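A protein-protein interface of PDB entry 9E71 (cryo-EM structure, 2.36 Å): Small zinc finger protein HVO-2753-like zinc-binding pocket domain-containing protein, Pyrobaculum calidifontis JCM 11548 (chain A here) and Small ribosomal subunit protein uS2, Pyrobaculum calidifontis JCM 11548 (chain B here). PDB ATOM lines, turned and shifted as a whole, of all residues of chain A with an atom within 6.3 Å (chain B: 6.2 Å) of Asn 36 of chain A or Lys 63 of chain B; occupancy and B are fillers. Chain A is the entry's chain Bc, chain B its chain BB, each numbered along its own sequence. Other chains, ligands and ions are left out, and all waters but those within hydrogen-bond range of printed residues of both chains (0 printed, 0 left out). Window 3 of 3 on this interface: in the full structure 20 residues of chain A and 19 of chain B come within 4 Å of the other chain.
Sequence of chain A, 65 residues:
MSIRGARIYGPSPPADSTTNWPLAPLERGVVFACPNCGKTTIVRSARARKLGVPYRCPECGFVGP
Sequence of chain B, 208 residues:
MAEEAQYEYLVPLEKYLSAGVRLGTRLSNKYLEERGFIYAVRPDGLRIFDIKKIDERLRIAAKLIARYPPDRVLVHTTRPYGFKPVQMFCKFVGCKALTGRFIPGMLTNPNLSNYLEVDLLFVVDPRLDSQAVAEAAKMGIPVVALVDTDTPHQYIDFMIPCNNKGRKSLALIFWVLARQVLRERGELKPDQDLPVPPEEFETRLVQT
NH2 of Arg 67 of chain B sits at hydrogen-bond distance from O of Pro 35 of chain A (2.8 Å).
The side-chain amino group (NZ) of Lys 63 of chain B sits at hydrogen-bond distance from the backbone carbonyl oxygen (O) of Asn 36 of chain A (2.4 Å).
The guanidinium group of Arg 67 of chain B sits close to the backbone NH of Gly 38 of chain A (3.4 Å).
NH2 of Arg 67 of chain B sits at hydrogen-bond distance from O of Cys 34 of chain A, 3.1 Å away.
The guanidinium group (NH1) of Arg 67 of chain B is in hydrogen-bond range of the backbone carbonyl oxygen (O) of Cys 37 of chain A (2.9 Å).
The backbone NH of Phe 62 of chain A sits close to the side-chain sulfur of Cys 60 of chain A (3.4 Å).
The side-chain sulfur (SG) of Cys 34 of chain A lies close to the backbone NH (N) of Asn 36 of chain A, 3.4 Å away.
NE of Arg 67 of chain B is in hydrogen-bond range of O of Lys 63 of chain B (3.3 Å).
The backbone NH (N) of Cys 57 of chain A is in hydrogen-bond range of the backbone carbonyl oxygen (O) of Phe 62 of chain A.
The side-chain amide nitrogen of Asn 36 of chain A lies close to the side-chain sulfur of Cys 60 of chain A (3.0 Å).
Among the printed residues, pairs that only touch across the chains: Pro 35 of chain A with Ile 60 of chain B, Pro 35 of chain A with Lys 63 of chain B, Pro 35 of chain A with Leu 64 of chain B, Asn 36 of chain A with Ile 60 of chain B and Phe 62 of chain A with Ile 60 of chain B.
Of the printed residues of chain B, Cys 34 of chain A touches Arg 67 (3.1 Å).
Of the printed residues of chain B, Pro 35 of chain A touches Ile 60, Lys 63, Leu 64 and Arg 67.
Asn 36 of chain A touches just these residues of chain B: Ile 60 and Lys 63.
Arg 59 of chain B touches none of the printed residues of chain A.
Lys 63 of chain B touches just these residues of chain A: Pro 35 and Asn 36.
Of the printed residues of chain A, Arg 67 of chain B touches Cys 34 (3.1 Å), Pro 35 (2.8 Å), Cys 37 (2.9 Å) and Gly 38 (3.3 Å).
Gln 180 of chain B touches none of the printed residues of chain A.
The nearest residue of chain B that does not touch Asn 36 of chain A is Arg 67 of chain B (4.4 Å).
The nearest residue of chain A that does not touch Lys 63 of chain B is Cys 37 of chain A (4.7 Å).
Hydrophobic or aromatic side chains of chain B within 4 Å of the printed part of chain A: Ile 60 and Leu 64.
Among the printed residues, 10 pairs touch across the chains.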
ATOM      1  N   ALA A  33     -29.463  13.904  -9.273  1.00  0.00           N
ATOM      2  CA  ALA A  33     -30.710  14.636  -9.409  1.00  0.00           C
ATOM      3  C   ALA A  33     -30.432  15.981 -10.059  1.00  0.00           C
ATOM      4  O   ALA A  33     -29.293  16.447 -10.074  1.00  0.00           O
ATOM      5  CB  ALA A  33     -31.385  14.837  -8.053  1.00  0.00           C
ATOM      6  N   CYS A  34     -31.484  16.601 -10.599  1.00  0.00           N
ATOM      7  CA  CYS A  34     -31.342  17.866 -11.312  1.00  0.00           C
ATOM      8  C   CYS A  34     -30.802  18.959 -10.400  1.00  0.00           C
ATOM      9  O   CYS A  34     -31.378  19.229  -9.339  1.00  0.00           O
ATOM     10  CB  CYS A  34     -32.676  18.310 -11.906  1.00  0.00           C
ATOM     11  SG  CYS A  34     -32.613  19.973 -12.602  1.00  0.00           S
ATOM     12  N   PRO A  35     -29.679  19.580 -10.766  1.00  0.00           N
ATOM     13  CA  PRO A  35     -29.101  20.625  -9.906  1.00  0.00           C
ATOM     14  C   PRO A  35     -30.005  21.828  -9.704  1.00  0.00           C
ATOM     15  O   PRO A  35     -29.950  22.464  -8.646  1.00  0.00           O
ATOM     16  CB  PRO A  35     -27.808  20.995 -10.642  1.00  0.00           C
ATOM     17  CG  PRO A  35     -27.461  19.760 -11.410  1.00  0.00           C
ATOM     18  CD  PRO A  35     -28.777  19.215 -11.869  1.00  0.00           C
ATOM     19  N   ASN A  36     -30.844  22.156 -10.685  1.00  0.00           N
ATOM     20  CA  ASN A  36     -31.726  23.306 -10.530  1.00  0.00           C
ATOM     21  C   ASN A  36     -32.953  22.962  -9.697  1.00  0.00           C
ATOM     22  O   ASN A  36     -33.282  23.685  -8.752  1.00  0.00           O
ATOM     23  CB  ASN A  36     -32.143  23.836 -11.901  1.00  0.00           C
ATOM     24  CG  ASN A  36     -33.095  25.007 -11.805  1.00  0.00           C
ATOM     25  OD1 ASN A  36     -32.897  25.918 -11.003  1.00  0.00           O
ATOM     26  ND2 ASN A  36     -34.137  24.989 -12.623  1.00  0.00           N
ATOM     27  N   CYS A  37     -33.640  21.866 -10.024  1.00  0.00           N
ATOM     28  CA  CYS A  37     -34.798  21.413  -9.262  1.00  0.00           C
ATOM     29  C   CYS A  37     -34.458  20.327  -8.255  1.00  0.00           C
ATOM     30  O   CYS A  37     -34.727  20.483  -7.063  1.00  0.00           O
ATOM     31  CB  CYS A  37     -35.900  20.886 -10.193  1.00  0.00           C
ATOM     32  SG  CYS A  37     -36.014  21.650 -11.806  1.00  0.00           S
ATOM     33  N   GLY A  38     -33.866  19.228  -8.708  1.00  0.00           N
ATOM     34  CA  GLY A  38     -33.724  18.043  -7.894  1.00  0.00           C
ATOM     35  C   GLY A  38     -34.851  17.049  -8.038  1.00  0.00           C
ATOM     36  O   GLY A  38     -34.863  16.042  -7.321  1.00  0.00           O
ATOM     37  N   CYS A  57     -33.118  19.425 -18.340  1.00  0.00           N
ATOM     38  CA  CYS A  57     -34.142  18.947 -17.420  1.00  0.00           C
ATOM     39  C   CYS A  57     -35.479  18.847 -18.142  1.00  0.00           C
ATOM     40  O   CYS A  57     -35.872  19.787 -18.838  1.00  0.00           O
ATOM     41  CB  CYS A  57     -34.277  19.867 -16.211  1.00  0.00           C
ATOM     42  SG  CYS A  57     -35.464  19.265 -14.974  1.00  0.00           S
ATOM     43  N   CYS A  60     -37.449  21.632 -15.649  1.00  0.00           N
ATOM     44  CA  CYS A  60     -36.931  22.990 -15.704  1.00  0.00           C
ATOM     45  C   CYS A  60     -36.093  23.172 -16.963  1.00  0.00           C
ATOM     46  O   CYS A  60     -35.744  22.198 -17.634  1.00  0.00           O
ATOM     47  CB  CYS A  60     -36.085  23.311 -14.473  1.00  0.00           C
ATOM     48  SG  CYS A  60     -34.375  22.771 -14.602  1.00  0.00           S
ATOM     49  N   GLY A  61     -35.781  24.424 -17.283  1.00  0.00           N
ATOM     50  CA  GLY A  61     -34.974  24.723 -18.449  1.00  0.00           C
ATOM     51  C   GLY A  61     -33.491  24.875 -18.177  1.00  0.00           C
ATOM     52  O   GLY A  61     -32.879  25.852 -18.619  1.00  0.00           O
ATOM     53  N   PHE A  62     -32.897  23.926 -17.458  1.00  0.00           N
ATOM     54  CA  PHE A  62     -31.490  23.997 -17.086  1.00  0.00           C
ATOM     55  C   PHE A  62     -30.678  23.030 -17.932  1.00  0.00           C
ATOM     56  O   PHE A  62     -31.013  21.844 -18.022  1.00  0.00           O
ATOM     57  CB  PHE A  62     -31.295  23.687 -15.602  1.00  0.00           C
ATOM     58  CG  PHE A  62     -29.868  23.438 -15.207  1.00  0.00           C
ATOM     59  CD1 PHE A  62     -28.991  24.491 -15.039  1.00  0.00           C
ATOM     60  CD2 PHE A  62     -29.413  22.153 -14.968  1.00  0.00           C
ATOM     61  CE1 PHE A  62     -27.685  24.268 -14.666  1.00  0.00           C
ATOM     62  CE2 PHE A  62     -28.107  21.925 -14.596  1.00  0.00           C
ATOM     63  CZ  PHE A  62     -27.243  22.984 -14.444  1.00  0.00           C
ATOM     64  N   LEU B  58     -23.568  29.692  -9.056  1.00  0.00           N
ATOM     65  CA  LEU B  58     -23.301  29.573  -7.623  1.00  0.00           C
ATOM     66  C   LEU B  58     -24.547  29.124  -6.873  1.00  0.00           C
ATOM     67  O   LEU B  58     -24.478  28.256  -5.995  1.00  0.00           O
ATOM     68  CB  LEU B  58     -22.799  30.902  -7.054  1.00  0.00           C
ATOM     69  CG  LEU B  58     -21.515  31.529  -7.591  1.00  0.00           C
ATOM     70  CD1 LEU B  58     -20.932  32.495  -6.584  1.00  0.00           C
ATOM     71  CD2 LEU B  58     -20.512  30.457  -7.945  1.00  0.00           C
ATOM     72  N   ARG B  59     -25.699  29.700  -7.221  1.00  0.00           N
ATOM     73  CA  ARG B  59     -26.951  29.329  -6.565  1.00  0.00           C
ATOM     74  C   ARG B  59     -27.300  27.867  -6.822  1.00  0.00           C
ATOM     75  O   ARG B  59     -27.587  27.108  -5.885  1.00  0.00           O
ATOM     76  CB  ARG B  59     -28.078  30.240  -7.047  1.00  0.00           C
ATOM     77  CG  ARG B  59     -27.889  31.704  -6.697  1.00  0.00           C
ATOM     78  CD  ARG B  59     -29.066  32.535  -7.171  1.00  0.00           C
ATOM     79  NE  ARG B  59     -28.818  33.963  -7.018  1.00  0.00           N
ATOM     80  CZ  ARG B  59     -29.526  34.768  -6.240  1.00  0.00           C
ATOM     81  NH1 ARG B  59     -30.555  34.323  -5.538  1.00  0.00           N
ATOM     82  NH2 ARG B  59     -29.190  36.052  -6.157  1.00  0.00           N
ATOM     83  N   ILE B  60     -27.260  27.451  -8.092  1.00  0.00           N
ATOM     84  CA  ILE B  60     -27.600  26.072  -8.431  1.00  0.00           C
ATOM     85  C   ILE B  60     -26.596  25.097  -7.835  1.00  0.00           C
ATOM     86  O   ILE B  60     -26.968  24.003  -7.391  1.00  0.00           O
ATOM     87  CB  ILE B  60     -27.704  25.909  -9.957  1.00  0.00           C
ATOM     88  CG1 ILE B  60     -28.714  26.905 -10.524  1.00  0.00           C
ATOM     89  CG2 ILE B  60     -28.087  24.490 -10.308  1.00  0.00           C
ATOM     90  CD1 ILE B  60     -28.650  27.052 -12.017  1.00  0.00           C
ATOM     91  N   ALA B  61     -25.319  25.477  -7.788  1.00  0.00           N
ATOM     92  CA  ALA B  61     -24.312  24.625  -7.174  1.00  0.00           C
ATOM     93  C   ALA B  61     -24.559  24.462  -5.684  1.00  0.00           C
ATOM     94  O   ALA B  61     -24.434  23.353  -5.151  1.00  0.00           O
ATOM     95  CB  ALA B  61     -22.920  25.200  -7.427  1.00  0.00           C
ATOM     96  N   ALA B  62     -24.901  25.557  -4.997  1.00  0.00           N
ATOM     97  CA  ALA B  62     -25.199  25.480  -3.572  1.00  0.00           C
ATOM     98  C   ALA B  62     -26.393  24.574  -3.314  1.00  0.00           C
ATOM     99  O   ALA B  62     -26.382  23.780  -2.368  1.00  0.00           O
ATOM    100  CB  ALA B  62     -25.451  26.877  -3.013  1.00  0.00           C
ATOM    101  N   LYS B  63     -27.414  24.655  -4.174  1.00  0.00           N
ATOM    102  CA  LYS B  63     -28.525  23.710  -4.083  1.00  0.00           C
ATOM    103  C   LYS B  63     -28.056  22.278  -4.314  1.00  0.00           C
ATOM    104  O   LYS B  63     -28.602  21.336  -3.728  1.00  0.00           O
ATOM    105  CB  LYS B  63     -29.619  24.072  -5.086  1.00  0.00           C
ATOM    106  CG  LYS B  63     -30.016  25.530  -5.081  1.00  0.00           C
ATOM    107  CD  LYS B  63     -31.491  25.691  -5.380  1.00  0.00           C
ATOM    108  CE  LYS B  63     -31.727  25.852  -6.871  1.00  0.00           C
ATOM    109  NZ  LYS B  63     -33.143  25.593  -7.237  1.00  0.00           N
ATOM    110  N   LEU B  64     -27.054  22.091  -5.175  1.00  0.00           N
ATOM    111  CA  LEU B  64     -26.555  20.745  -5.440  1.00  0.00           C
ATOM    112  C   LEU B  64     -25.851  20.153  -4.220  1.00  0.00           C
ATOM    113  O   LEU B  64     -26.152  19.028  -3.807  1.00  0.00           O
ATOM    114  CB  LEU B  64     -25.619  20.762  -6.645  1.00  0.00           C
ATOM    115  CG  LEU B  64     -25.177  19.380  -7.124  1.00  0.00           C
ATOM    116  CD1 LEU B  64     -26.310  18.373  -6.987  1.00  0.00           C
ATOM    117  CD2 LEU B  64     -24.698  19.450  -8.555  1.00  0.00           C
ATOM    118  N   ILE B  65     -24.904  20.893  -3.633  1.00  0.00           N
ATOM    119  CA  ILE B  65     -24.218  20.385  -2.439  1.00  0.00           C
ATOM    120  C   ILE B  65     -25.171  20.290  -1.249  1.00  0.00           C
ATOM    121  O   ILE B  65     -24.967  19.469  -0.346  1.00  0.00           O
ATOM    122  CB  ILE B  65     -22.947  21.198  -2.089  1.00  0.00           C
ATOM    123  CG1 ILE B  65     -21.894  21.182  -3.206  1.00  0.00           C
ATOM    124  CG2 ILE B  65     -22.304  20.713  -0.801  1.00  0.00           C
ATOM    125  CD1 ILE B  65     -21.884  22.319  -4.154  1.00  0.00           C
ATOM    126  N   ALA B  66     -26.234  21.102  -1.233  1.00  0.00           N
ATOM    127  CA  ALA B  66     -27.172  21.053  -0.113  1.00  0.00           C
ATOM    128  C   ALA B  66     -27.902  19.716  -0.041  1.00  0.00           C
ATOM    129  O   ALA B  66     -28.240  19.246   1.050  1.00  0.00           O
ATOM    130  CB  ALA B  66     -28.175  22.198  -0.222  1.00  0.00           C
ATOM    131  N   ARG B  67     -28.139  19.082  -1.185  1.00  0.00           N
ATOM    132  CA  ARG B  67     -28.908  17.843  -1.214  1.00  0.00           C
ATOM    133  C   ARG B  67     -28.096  16.615  -0.836  1.00  0.00           C
ATOM    134  O   ARG B  67     -28.675  15.533  -0.706  1.00  0.00           O
ATOM    135  CB  ARG B  67     -29.528  17.661  -2.598  1.00  0.00           C
ATOM    136  CG  ARG B  67     -30.776  18.496  -2.793  1.00  0.00           C
ATOM    137  CD  ARG B  67     -31.333  18.363  -4.188  1.00  0.00           C
ATOM    138  NE  ARG B  67     -30.412  18.934  -5.159  1.00  0.00           N
ATOM    139  CZ  ARG B  67     -30.746  19.852  -6.054  1.00  0.00           C
ATOM    140  NH1 ARG B  67     -31.983  20.310  -6.147  1.00  0.00           N
ATOM    141  NH2 ARG B  67     -29.811  20.333  -6.865  1.00  0.00           N
ATOM    142  N   TYR B  68     -26.790  16.745  -0.653  1.00  0.00           N
ATOM    143  CA  TYR B  68     -25.964  15.619  -0.266  1.00  0.00           C
ATOM    144  C   TYR B  68     -25.648  15.696   1.215  1.00  0.00           C
ATOM    145  O   TYR B  68     -25.555  16.805   1.758  1.00  0.00           O
ATOM    146  CB  TYR B  68     -24.661  15.601  -1.074  1.00  0.00           C
ATOM    147  CG  TYR B  68     -24.842  15.182  -2.513  1.00  0.00           C
ATOM    148  CD1 TYR B  68     -24.766  13.845  -2.879  1.00  0.00           C
ATOM    149  CD2 TYR B  68     -25.101  16.117  -3.502  1.00  0.00           C
ATOM    150  CE1 TYR B  68     -24.938  13.455  -4.188  1.00  0.00           C
ATOM    151  CE2 TYR B  68     -25.274  15.736  -4.815  1.00  0.00           C
ATOM    152  CZ  TYR B  68     -25.191  14.403  -5.152  1.00  0.00           C
ATOM    153  OH  TYR B  68     -25.361  14.015  -6.458  1.00  0.00           O
ATOM    154  N   GLN B 180     -24.406  30.030   1.002  1.00  0.00           N
ATOM    155  CA  GLN B 180     -25.602  29.517   0.340  1.00  0.00           C
ATOM    156  C   GLN B 180     -25.879  28.069   0.725  1.00  0.00           C
ATOM    157  O   GLN B 180     -27.040  27.671   0.862  1.00  0.00           O
ATOM    158  CB  GLN B 180     -25.478  29.647  -1.173  1.00  0.00           C
ATOM    159  CG  GLN B 180     -26.819  29.757  -1.876  1.00  0.00           C
ATOM    160  CD  GLN B 180     -27.355  31.175  -1.898  1.00  0.00           C
ATOM    161  OE1 GLN B 180     -26.718  32.099  -1.396  1.00  0.00           O
ATOM    162  NE2 GLN B 180     -28.531  31.354  -2.488  1.00  0.00           N
ATOM    163  N   VAL B 181     -24.831  27.259   0.899  1.00  0.00           N
ATOM    164  CA  VAL B 181     -25.055  25.873   1.292  1.00  0.00           C
ATOM    165  C   VAL B 181     -25.593  25.809   2.713  1.00  0.00           C
ATOM    166  O   VAL B 181     -26.458  24.983   3.019  1.00  0.00           O
ATOM    167  CB  VAL B 181     -23.776  25.029   1.103  1.00  0.00           C
ATOM    168  CG1 VAL B 181     -22.747  25.276   2.198  1.00  0.00           C
ATOM    169  CG2 VAL B 181     -24.129  23.559   1.032  1.00  0.00           C
ATOM    170  N   GLU B 184     -29.273  26.741   2.443  1.00  0.00           N
ATOM    171  CA  GLU B 184     -30.076  25.665   1.869  1.00  0.00           C
ATOM    172  C   GLU B 184     -30.226  24.502   2.841  1.00  0.00           C
ATOM    173  O   GLU B 184     -31.290  23.874   2.903  1.00  0.00           O
ATOM    174  CB  GLU B 184     -29.465  25.192   0.549  1.00  0.00           C
ATOM    175  CG  GLU B 184     -29.373  26.269  -0.530  1.00  0.00           C
ATOM    176  CD  GLU B 184     -30.719  26.593  -1.147  1.00  0.00           C
ATOM    177  OE1 GLU B 184     -31.121  25.922  -2.121  1.00  0.00           O
ATOM    178  OE2 GLU B 184     -31.383  27.522  -0.648  1.00  0.00           O
